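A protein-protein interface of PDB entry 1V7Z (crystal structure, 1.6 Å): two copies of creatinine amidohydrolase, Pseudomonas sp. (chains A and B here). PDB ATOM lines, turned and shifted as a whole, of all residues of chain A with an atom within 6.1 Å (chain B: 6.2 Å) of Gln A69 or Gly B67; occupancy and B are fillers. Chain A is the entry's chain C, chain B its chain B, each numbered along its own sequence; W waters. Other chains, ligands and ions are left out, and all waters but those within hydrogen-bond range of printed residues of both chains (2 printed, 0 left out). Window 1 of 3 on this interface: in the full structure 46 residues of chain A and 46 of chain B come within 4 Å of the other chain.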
ATOM      1  N   PRO A  29     -20.775   1.399  14.980  1.00  0.00           N
ATOM      2  CA  PRO A  29     -22.068   0.743  15.220  1.00  0.00           C
ATOM      3  C   PRO A  29     -21.971  -0.225  16.399  1.00  0.00           C
ATOM      4  O   PRO A  29     -20.970  -0.939  16.520  1.00  0.00           O
ATOM      5  CB  PRO A  29     -22.343  -0.012  13.911  1.00  0.00           C
ATOM      6  CG  PRO A  29     -21.328   0.489  12.937  1.00  0.00           C
ATOM      7  CD  PRO A  29     -20.168   0.959  13.714  1.00  0.00           C
ATOM      8  N   GLY A  31     -24.301  -3.160  18.126  1.00  0.00           N
ATOM      9  CA  GLY A  31     -25.501  -3.949  17.935  1.00  0.00           C
ATOM     10  C   GLY A  31     -25.676  -5.088  18.922  1.00  0.00           C
ATOM     11  O   GLY A  31     -25.405  -4.959  20.124  1.00  0.00           O
ATOM     12  N   ALA A  32     -26.150  -6.201  18.380  1.00  0.00           N
ATOM     13  CA  ALA A  32     -26.521  -7.397  19.132  1.00  0.00           C
ATOM     14  C   ALA A  32     -26.849  -8.536  18.176  1.00  0.00           C
ATOM     15  O   ALA A  32     -27.140  -8.320  16.990  1.00  0.00           O
ATOM     16  CB  ALA A  32     -27.733  -7.117  20.023  1.00  0.00           C
ATOM     17  N   LEU A  33     -26.777  -9.750  18.705  1.00  0.00           N
ATOM     18  CA  LEU A  33     -27.348 -10.936  18.080  1.00  0.00           C
ATOM     19  C   LEU A  33     -28.523 -11.332  18.953  1.00  0.00           C
ATOM     20  O   LEU A  33     -28.345 -11.752  20.095  1.00  0.00           O
ATOM     21  CB  LEU A  33     -26.323 -12.068  17.998  1.00  0.00           C
ATOM     22  CG  LEU A  33     -26.784 -13.346  17.282  1.00  0.00           C
ATOM     23  CD1 LEU A  33     -27.044 -13.088  15.803  1.00  0.00           C
ATOM     24  CD2 LEU A  33     -25.770 -14.478  17.454  1.00  0.00           C
ATOM     25  N   VAL A  46     -27.193  -5.092  14.349  1.00  0.00           N
ATOM     26  CA  VAL A  46     -25.925  -4.720  13.712  1.00  0.00           C
ATOM     27  C   VAL A  46     -26.172  -4.126  12.323  1.00  0.00           C
ATOM     28  O   VAL A  46     -25.640  -3.070  12.000  1.00  0.00           O
ATOM     29  CB  VAL A  46     -24.973  -5.929  13.564  1.00  0.00           C
ATOM     30  CG1 VAL A  46     -23.706  -5.533  12.791  1.00  0.00           C
ATOM     31  CG2 VAL A  46     -24.625  -6.515  14.917  1.00  0.00           C
ATOM     32  N   PRO A  66     -15.487  -1.304  12.346  1.00  0.00           N
ATOM     33  CA  PRO A  66     -16.194  -2.581  12.461  1.00  0.00           C
ATOM     34  C   PRO A  66     -17.164  -2.566  13.641  1.00  0.00           C
ATOM     35  O   PRO A  66     -16.822  -2.086  14.726  1.00  0.00           O
ATOM     36  CB  PRO A  66     -15.065  -3.591  12.683  1.00  0.00           C
ATOM     37  CG  PRO A  66     -13.875  -2.950  12.080  1.00  0.00           C
ATOM     38  CD  PRO A  66     -14.023  -1.483  12.304  1.00  0.00           C
ATOM     39  N   GLY A  67     -18.356  -3.095  13.420  1.00  0.00           N
ATOM     40  CA  GLY A  67     -19.422  -3.007  14.408  1.00  0.00           C
ATOM     41  C   GLY A  67     -19.246  -4.002  15.537  1.00  0.00           C
ATOM     42  O   GLY A  67     -18.623  -5.053  15.370  1.00  0.00           O
ATOM     43  N   LEU A  68     -19.792  -3.660  16.696  1.00  0.00           N
ATOM     44  CA  LEU A  68     -19.875  -4.601  17.800  1.00  0.00           C
ATOM     45  C   LEU A  68     -21.075  -5.494  17.520  1.00  0.00           C
ATOM     46  O   LEU A  68     -22.203  -5.028  17.379  1.00  0.00           O
ATOM     47  CB  LEU A  68     -19.985  -3.864  19.138  1.00  0.00           C
ATOM     48  CG  LEU A  68     -18.853  -2.867  19.452  1.00  0.00           C
ATOM     49  CD1 LEU A  68     -18.839  -2.501  20.920  1.00  0.00           C
ATOM     50  CD2 LEU A  68     -17.498  -3.400  19.033  1.00  0.00           C
ATOM     51  N   GLN A  69     -20.799  -6.788  17.401  1.00  0.00           N
ATOM     52  CA  GLN A  69     -21.744  -7.782  16.921  1.00  0.00           C
ATOM     53  C   GLN A  69     -22.598  -8.354  18.042  1.00  0.00           C
ATOM     54  O   GLN A  69     -23.668  -8.910  17.786  1.00  0.00           O
ATOM     55  CB  GLN A  69     -20.988  -8.937  16.256  1.00  0.00           C
ATOM     56  CG  GLN A  69     -19.931  -8.535  15.234  1.00  0.00           C
ATOM     57  CD  GLN A  69     -20.533  -8.054  13.932  1.00  0.00           C
ATOM     58  OE1 GLN A  69     -21.304  -8.775  13.290  1.00  0.00           O
ATOM     59  NE2 GLN A  69     -20.196  -6.827  13.543  1.00  0.00           N
ATOM     60  N   TYR A  70     -22.089  -8.247  19.269  1.00  0.00           N
ATOM     61  CA  TYR A  70     -22.721  -8.809  20.451  1.00  0.00           C
ATOM     62  C   TYR A  70     -22.896  -7.695  21.464  1.00  0.00           C
ATOM     63  O   TYR A  70     -21.975  -6.921  21.713  1.00  0.00           O
ATOM     64  CB  TYR A  70     -21.857  -9.927  21.050  1.00  0.00           C
ATOM     65  CG  TYR A  70     -21.617 -11.084  20.113  1.00  0.00           C
ATOM     66  CD1 TYR A  70     -20.496 -11.120  19.295  1.00  0.00           C
ATOM     67  CD2 TYR A  70     -22.511 -12.147  20.037  1.00  0.00           C
ATOM     68  CE1 TYR A  70     -20.275 -12.171  18.427  1.00  0.00           C
ATOM     69  CE2 TYR A  70     -22.301 -13.201  19.166  1.00  0.00           C
ATOM     70  CZ  TYR A  70     -21.175 -13.213  18.365  1.00  0.00           C
ATOM     71  OH  TYR A  70     -20.962 -14.266  17.502  1.00  0.00           O
ATOM     72  N   GLY A  71     -24.096  -7.615  22.032  1.00  0.00           N
ATOM     73  CA  GLY A  71     -24.458  -6.567  22.961  1.00  0.00           C
ATOM     74  C   GLY A  71     -24.988  -7.107  24.275  1.00  0.00           C
ATOM     75  O   GLY A  71     -24.931  -8.314  24.544  1.00  0.00           O
ATOM     76  N   THR A  88     -27.591 -13.963  21.846  1.00  0.00           N
ATOM     77  CA  THR A  88     -26.274 -14.288  22.382  1.00  0.00           C
ATOM     78  C   THR A  88     -25.678 -13.018  22.959  1.00  0.00           C
ATOM     79  O   THR A  88     -25.210 -12.152  22.218  1.00  0.00           O
ATOM     80  CB  THR A  88     -25.364 -14.835  21.266  1.00  0.00           C
ATOM     81  OG1 THR A  88     -25.962 -15.997  20.674  1.00  0.00           O
ATOM     82  CG2 THR A  88     -24.042 -15.326  21.835  1.00  0.00           C
ATOM     83  N   LEU B  28     -17.234 -20.023  15.062  1.00  0.00           N
ATOM     84  CA  LEU B  28     -17.046 -18.616  15.440  1.00  0.00           C
ATOM     85  C   LEU B  28     -15.702 -18.124  14.903  1.00  0.00           C
ATOM     86  O   LEU B  28     -14.648 -18.527  15.410  1.00  0.00           O
ATOM     87  CB  LEU B  28     -17.077 -18.463  16.962  1.00  0.00           C
ATOM     88  CG  LEU B  28     -16.762 -17.077  17.543  1.00  0.00           C
ATOM     89  CD1 LEU B  28     -17.783 -16.073  17.059  1.00  0.00           C
ATOM     90  CD2 LEU B  28     -16.695 -17.111  19.063  1.00  0.00           C
ATOM     91  N   PRO B  29     -15.726 -17.268  13.883  1.00  0.00           N
ATOM     92  CA  PRO B  29     -14.502 -16.609  13.420  1.00  0.00           C
ATOM     93  C   PRO B  29     -13.998 -15.607  14.448  1.00  0.00           C
ATOM     94  O   PRO B  29     -14.801 -14.872  15.031  1.00  0.00           O
ATOM     95  CB  PRO B  29     -14.934 -15.893  12.129  1.00  0.00           C
ATOM     96  CG  PRO B  29     -16.290 -16.415  11.807  1.00  0.00           C
ATOM     97  CD  PRO B  29     -16.897 -16.880  13.082  1.00  0.00           C
ATOM     98  N   VAL B  30     -12.688 -15.594  14.677  1.00  0.00           N
ATOM     99  CA  VAL B  30     -12.075 -14.673  15.619  1.00  0.00           C
ATOM    100  C   VAL B  30     -10.934 -13.943  14.921  1.00  0.00           C
ATOM    101  O   VAL B  30      -9.883 -14.525  14.644  1.00  0.00           O
ATOM    102  CB  VAL B  30     -11.538 -15.390  16.872  1.00  0.00           C
ATOM    103  CG1 VAL B  30     -11.084 -14.377  17.912  1.00  0.00           C
ATOM    104  CG2 VAL B  30     -12.595 -16.328  17.436  1.00  0.00           C
ATOM    105  N   GLY B  31     -11.145 -12.666  14.648  1.00  0.00           N
ATOM    106  CA  GLY B  31     -10.213 -11.877  13.867  1.00  0.00           C
ATOM    107  C   GLY B  31      -9.565 -10.718  14.596  1.00  0.00           C
ATOM    108  O   GLY B  31      -9.190 -10.807  15.762  1.00  0.00           O
ATOM    109  N   VAL B  46     -10.514 -10.878   9.938  1.00  0.00           N
ATOM    110  CA  VAL B  46     -11.935 -11.249  10.020  1.00  0.00           C
ATOM    111  C   VAL B  46     -12.421 -11.865   8.715  1.00  0.00           C
ATOM    112  O   VAL B  46     -13.042 -12.922   8.716  1.00  0.00           O
ATOM    113  CB  VAL B  46     -12.844 -10.030  10.323  1.00  0.00           C
ATOM    114  CG1 VAL B  46     -14.326 -10.457  10.371  1.00  0.00           C
ATOM    115  CG2 VAL B  46     -12.420  -9.354  11.610  1.00  0.00           C
ATOM    116  N   THR B  50     -13.708 -15.941   8.211  1.00  0.00           N
ATOM    117  CA  THR B  50     -15.145 -15.934   7.956  1.00  0.00           C
ATOM    118  C   THR B  50     -15.467 -16.626   6.632  1.00  0.00           C
ATOM    119  O   THR B  50     -16.407 -17.412   6.547  1.00  0.00           O
ATOM    120  CB  THR B  50     -15.682 -14.496   7.984  1.00  0.00           C
ATOM    121  OG1 THR B  50     -15.468 -13.937   9.287  1.00  0.00           O
ATOM    122  CG2 THR B  50     -17.191 -14.466   7.800  1.00  0.00           C
ATOM    123  N   MET B  65     -21.374 -18.203  13.483  1.00  0.00           N
ATOM    124  CA  MET B  65     -21.724 -17.074  14.335  1.00  0.00           C
ATOM    125  C   MET B  65     -21.096 -15.776  13.826  1.00  0.00           C
ATOM    126  O   MET B  65     -20.091 -15.815  13.114  1.00  0.00           O
ATOM    127  CB  MET B  65     -21.226 -17.340  15.756  1.00  0.00           C
ATOM    128  CG  MET B  65     -21.898 -18.523  16.437  1.00  0.00           C
ATOM    129  SD  MET B  65     -23.574 -18.123  16.947  1.00  0.00           S
ATOM    130  CE  MET B  65     -23.291 -17.052  18.354  1.00  0.00           C
ATOM    131  N   PRO B  66     -21.658 -14.626  14.203  1.00  0.00           N
ATOM    132  CA  PRO B  66     -20.999 -13.347  13.923  1.00  0.00           C
ATOM    133  C   PRO B  66     -19.561 -13.337  14.436  1.00  0.00           C
ATOM    134  O   PRO B  66     -19.294 -13.762  15.559  1.00  0.00           O
ATOM    135  CB  PRO B  66     -21.876 -12.326  14.660  1.00  0.00           C
ATOM    136  CG  PRO B  66     -23.220 -12.968  14.705  1.00  0.00           C
ATOM    137  CD  PRO B  66     -22.945 -14.434  14.895  1.00  0.00           C
ATOM    138  N   GLY B  67     -18.637 -12.873  13.608  1.00  0.00           N
ATOM    139  CA  GLY B  67     -17.230 -12.910  13.944  1.00  0.00           C
ATOM    140  C   GLY B  67     -16.803 -11.868  14.957  1.00  0.00           C
ATOM    141  O   GLY B  67     -17.410 -10.796  15.074  1.00  0.00           O
ATOM    142  N   LEU B  68     -15.772 -12.195  15.723  1.00  0.00           N
ATOM    143  CA  LEU B  68     -15.107 -11.222  16.572  1.00  0.00           C
ATOM    144  C   LEU B  68     -14.218 -10.343  15.690  1.00  0.00           C
ATOM    145  O   LEU B  68     -13.303 -10.824  15.017  1.00  0.00           O
ATOM    146  CB  LEU B  68     -14.324 -11.909  17.697  1.00  0.00           C
ATOM    147  CG  LEU B  68     -15.177 -12.847  18.583  1.00  0.00           C
ATOM    148  CD1 LEU B  68     -14.419 -13.232  19.829  1.00  0.00           C
ATOM    149  CD2 LEU B  68     -16.519 -12.245  18.971  1.00  0.00           C
ATOM    150  N   GLN B  69     -14.532  -9.053  15.688  1.00  0.00           N
ATOM    151  CA  GLN B  69     -13.927  -8.070  14.788  1.00  0.00           C
ATOM    152  C   GLN B  69     -12.637  -7.478  15.320  1.00  0.00           C
ATOM    153  O   GLN B  69     -11.835  -6.955  14.542  1.00  0.00           O
ATOM    154  CB  GLN B  69     -14.904  -6.911  14.539  1.00  0.00           C
ATOM    155  CG  GLN B  69     -16.347  -7.329  14.246  1.00  0.00           C
ATOM    156  CD  GLN B  69     -16.520  -7.896  12.859  1.00  0.00           C
ATOM    157  OE1 GLN B  69     -16.212  -7.219  11.868  1.00  0.00           O
ATOM    158  NE2 GLN B  69     -17.041  -9.116  12.772  1.00  0.00           N
ATOM    159  N   TYR B  70     -12.463  -7.522  16.639  1.00  0.00           N
ATOM    160  CA  TYR B  70     -11.325  -6.915  17.323  1.00  0.00           C
ATOM    161  C   TYR B  70     -10.620  -7.995  18.134  1.00  0.00           C
ATOM    162  O   TYR B  70     -11.267  -8.757  18.854  1.00  0.00           O
ATOM    163  CB  TYR B  70     -11.784  -5.791  18.247  1.00  0.00           C
ATOM    164  CG  TYR B  70     -12.480  -4.656  17.533  1.00  0.00           C
ATOM    165  CD1 TYR B  70     -13.860  -4.659  17.353  1.00  0.00           C
ATOM    166  CD2 TYR B  70     -11.765  -3.572  17.060  1.00  0.00           C
ATOM    167  CE1 TYR B  70     -14.505  -3.610  16.696  1.00  0.00           C
ATOM    168  CE2 TYR B  70     -12.396  -2.523  16.405  1.00  0.00           C
ATOM    169  CZ  TYR B  70     -13.757  -2.543  16.232  1.00  0.00           C
ATOM    170  OH  TYR B  70     -14.377  -1.499  15.583  1.00  0.00           O
HETATM  171  O   HOH W   1     -20.236 -10.830  11.702  1.00  0.00           O
HETATM  172  O   HOH W   2     -17.943  -5.125  10.959  1.00  0.00           O
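The backbone carbonyl oxygen (O) of Pro A66 sits at hydrogen-bond distance from the side-chain hydroxyl (OH) of Tyr B70, at 2.7 Å. The backbone carbonyl oxygen (O) of Pro B66 lies within hydrogen-bond range of the side-chain hydroxyl (OH) of Tyr A70 (2.6 Å).
The backbone carbonyl oxygen (O) of Leu A68 lies within hydrogen-bond range of the backbone NH (N) of Gly A31 (2.9 Å). The backbone NH of Gly B31 lies within hydrogen-bond range of the backbone carbonyl oxygen of Leu B68 (2.9 Å). The backbone carbonyl oxygen of Pro A29 sits at hydrogen-bond distance from the backbone NH of Leu A68 (3.0 Å). O of Gly A67 lies within hydrogen-bond range of NE2 of Gln A69, at 3.0 Å. The backbone carbonyl oxygen (O) of Gln A69 is in hydrogen-bond range of the backbone NH (N) of Leu A33. The side-chain amide nitrogen (NE2) of Gln B69 lies within hydrogen-bond range of the backbone carbonyl oxygen (O) of Gly B67, at 2.9 Å.
Among the printed residues, pairs that only touch across the chains: Leu A33 with Met B65, Leu A33 with Pro B66, Pro A66 with Gln B69, Gly A67 with Gln B69, Leu A68 with Tyr B70, Gln A69 with Pro B66, Gln A69 with Gly B67, Gln A69 with Gln B69, Tyr A70 with Leu B28, Tyr A70 with Met B65, Tyr A70 with Leu B68 and Thr A88 with Met B65.
Pro A29 touches none of the printed residues of chain B. Of the printed residues of chain B, Leu A33 touches Met B65 and Pro B66. Of the printed residues of chain B, Gly A67 touches Gln B69. Of chain B, only Pro B66, Gly B67 and Gln B69 come within 4 Å of Gln A69. Of the printed residues of chain B, Tyr A70 touches Leu B28 (3.7 Å), Met B65 (3.5 Å), Pro B66 (2.6 Å) and Leu B68 (3.8 Å). Gly B67 touches just one residue of chain A: Gln A69 (3.4 Å). The nearest residue of chain B that does not touch Gln A69 is Leu B68 (5.6 Å). The nearest residue of chain A that does not touch Gly B67 is Tyr A70 (4.6 Å). The nearest printed residue of chain B that does not touch Gly A67 is Tyr B70 (4.6 Å).
Of the 12 printed residues of chain B, 7 touch a printed residue of chain A. Hydrophobic or aromatic side chains of chain B that line the printed part of chain A: Leu B28, Met B65, Pro B66, Leu B68 and Tyr B70. Of the 12 printed residues of chain A, 7 touch a printed residue of chain B. Printed residues of chain A that touch a printed residue of chain B: Leu A33, Pro A66, Gly A67, Leu A68, Gln A69, Tyr A70 and Thr A88. Hydrophobic or aromatic side chains of chain A that line the printed part of chain B: Leu A33, Pro A66, Leu A68 and Tyr A70. Among the printed residues, no Asp or Glu carboxylate lies within 4 Å of a Lys or Arg side-chain nitrogen of the other chain.
Pro A66 touches Gln B69, and with the chains exchanged Gln A69 touches Pro B66. Pro A66 touches Tyr B70, and with the chains exchanged Tyr A70 touches Pro B66. Leu A68 touches Tyr B70, and with the chains exchanged Tyr A70 touches Leu B68. Gln B69 touches its own counterpart, Gln A69. 8 positions are printed for both chains.
Water W1 bridges OE1 of Gln A69 (2.8 Å) and N of Gly B67 (3.2 Å). Water W2 bridges OE1 of Gln B69 and N of Gly A67.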
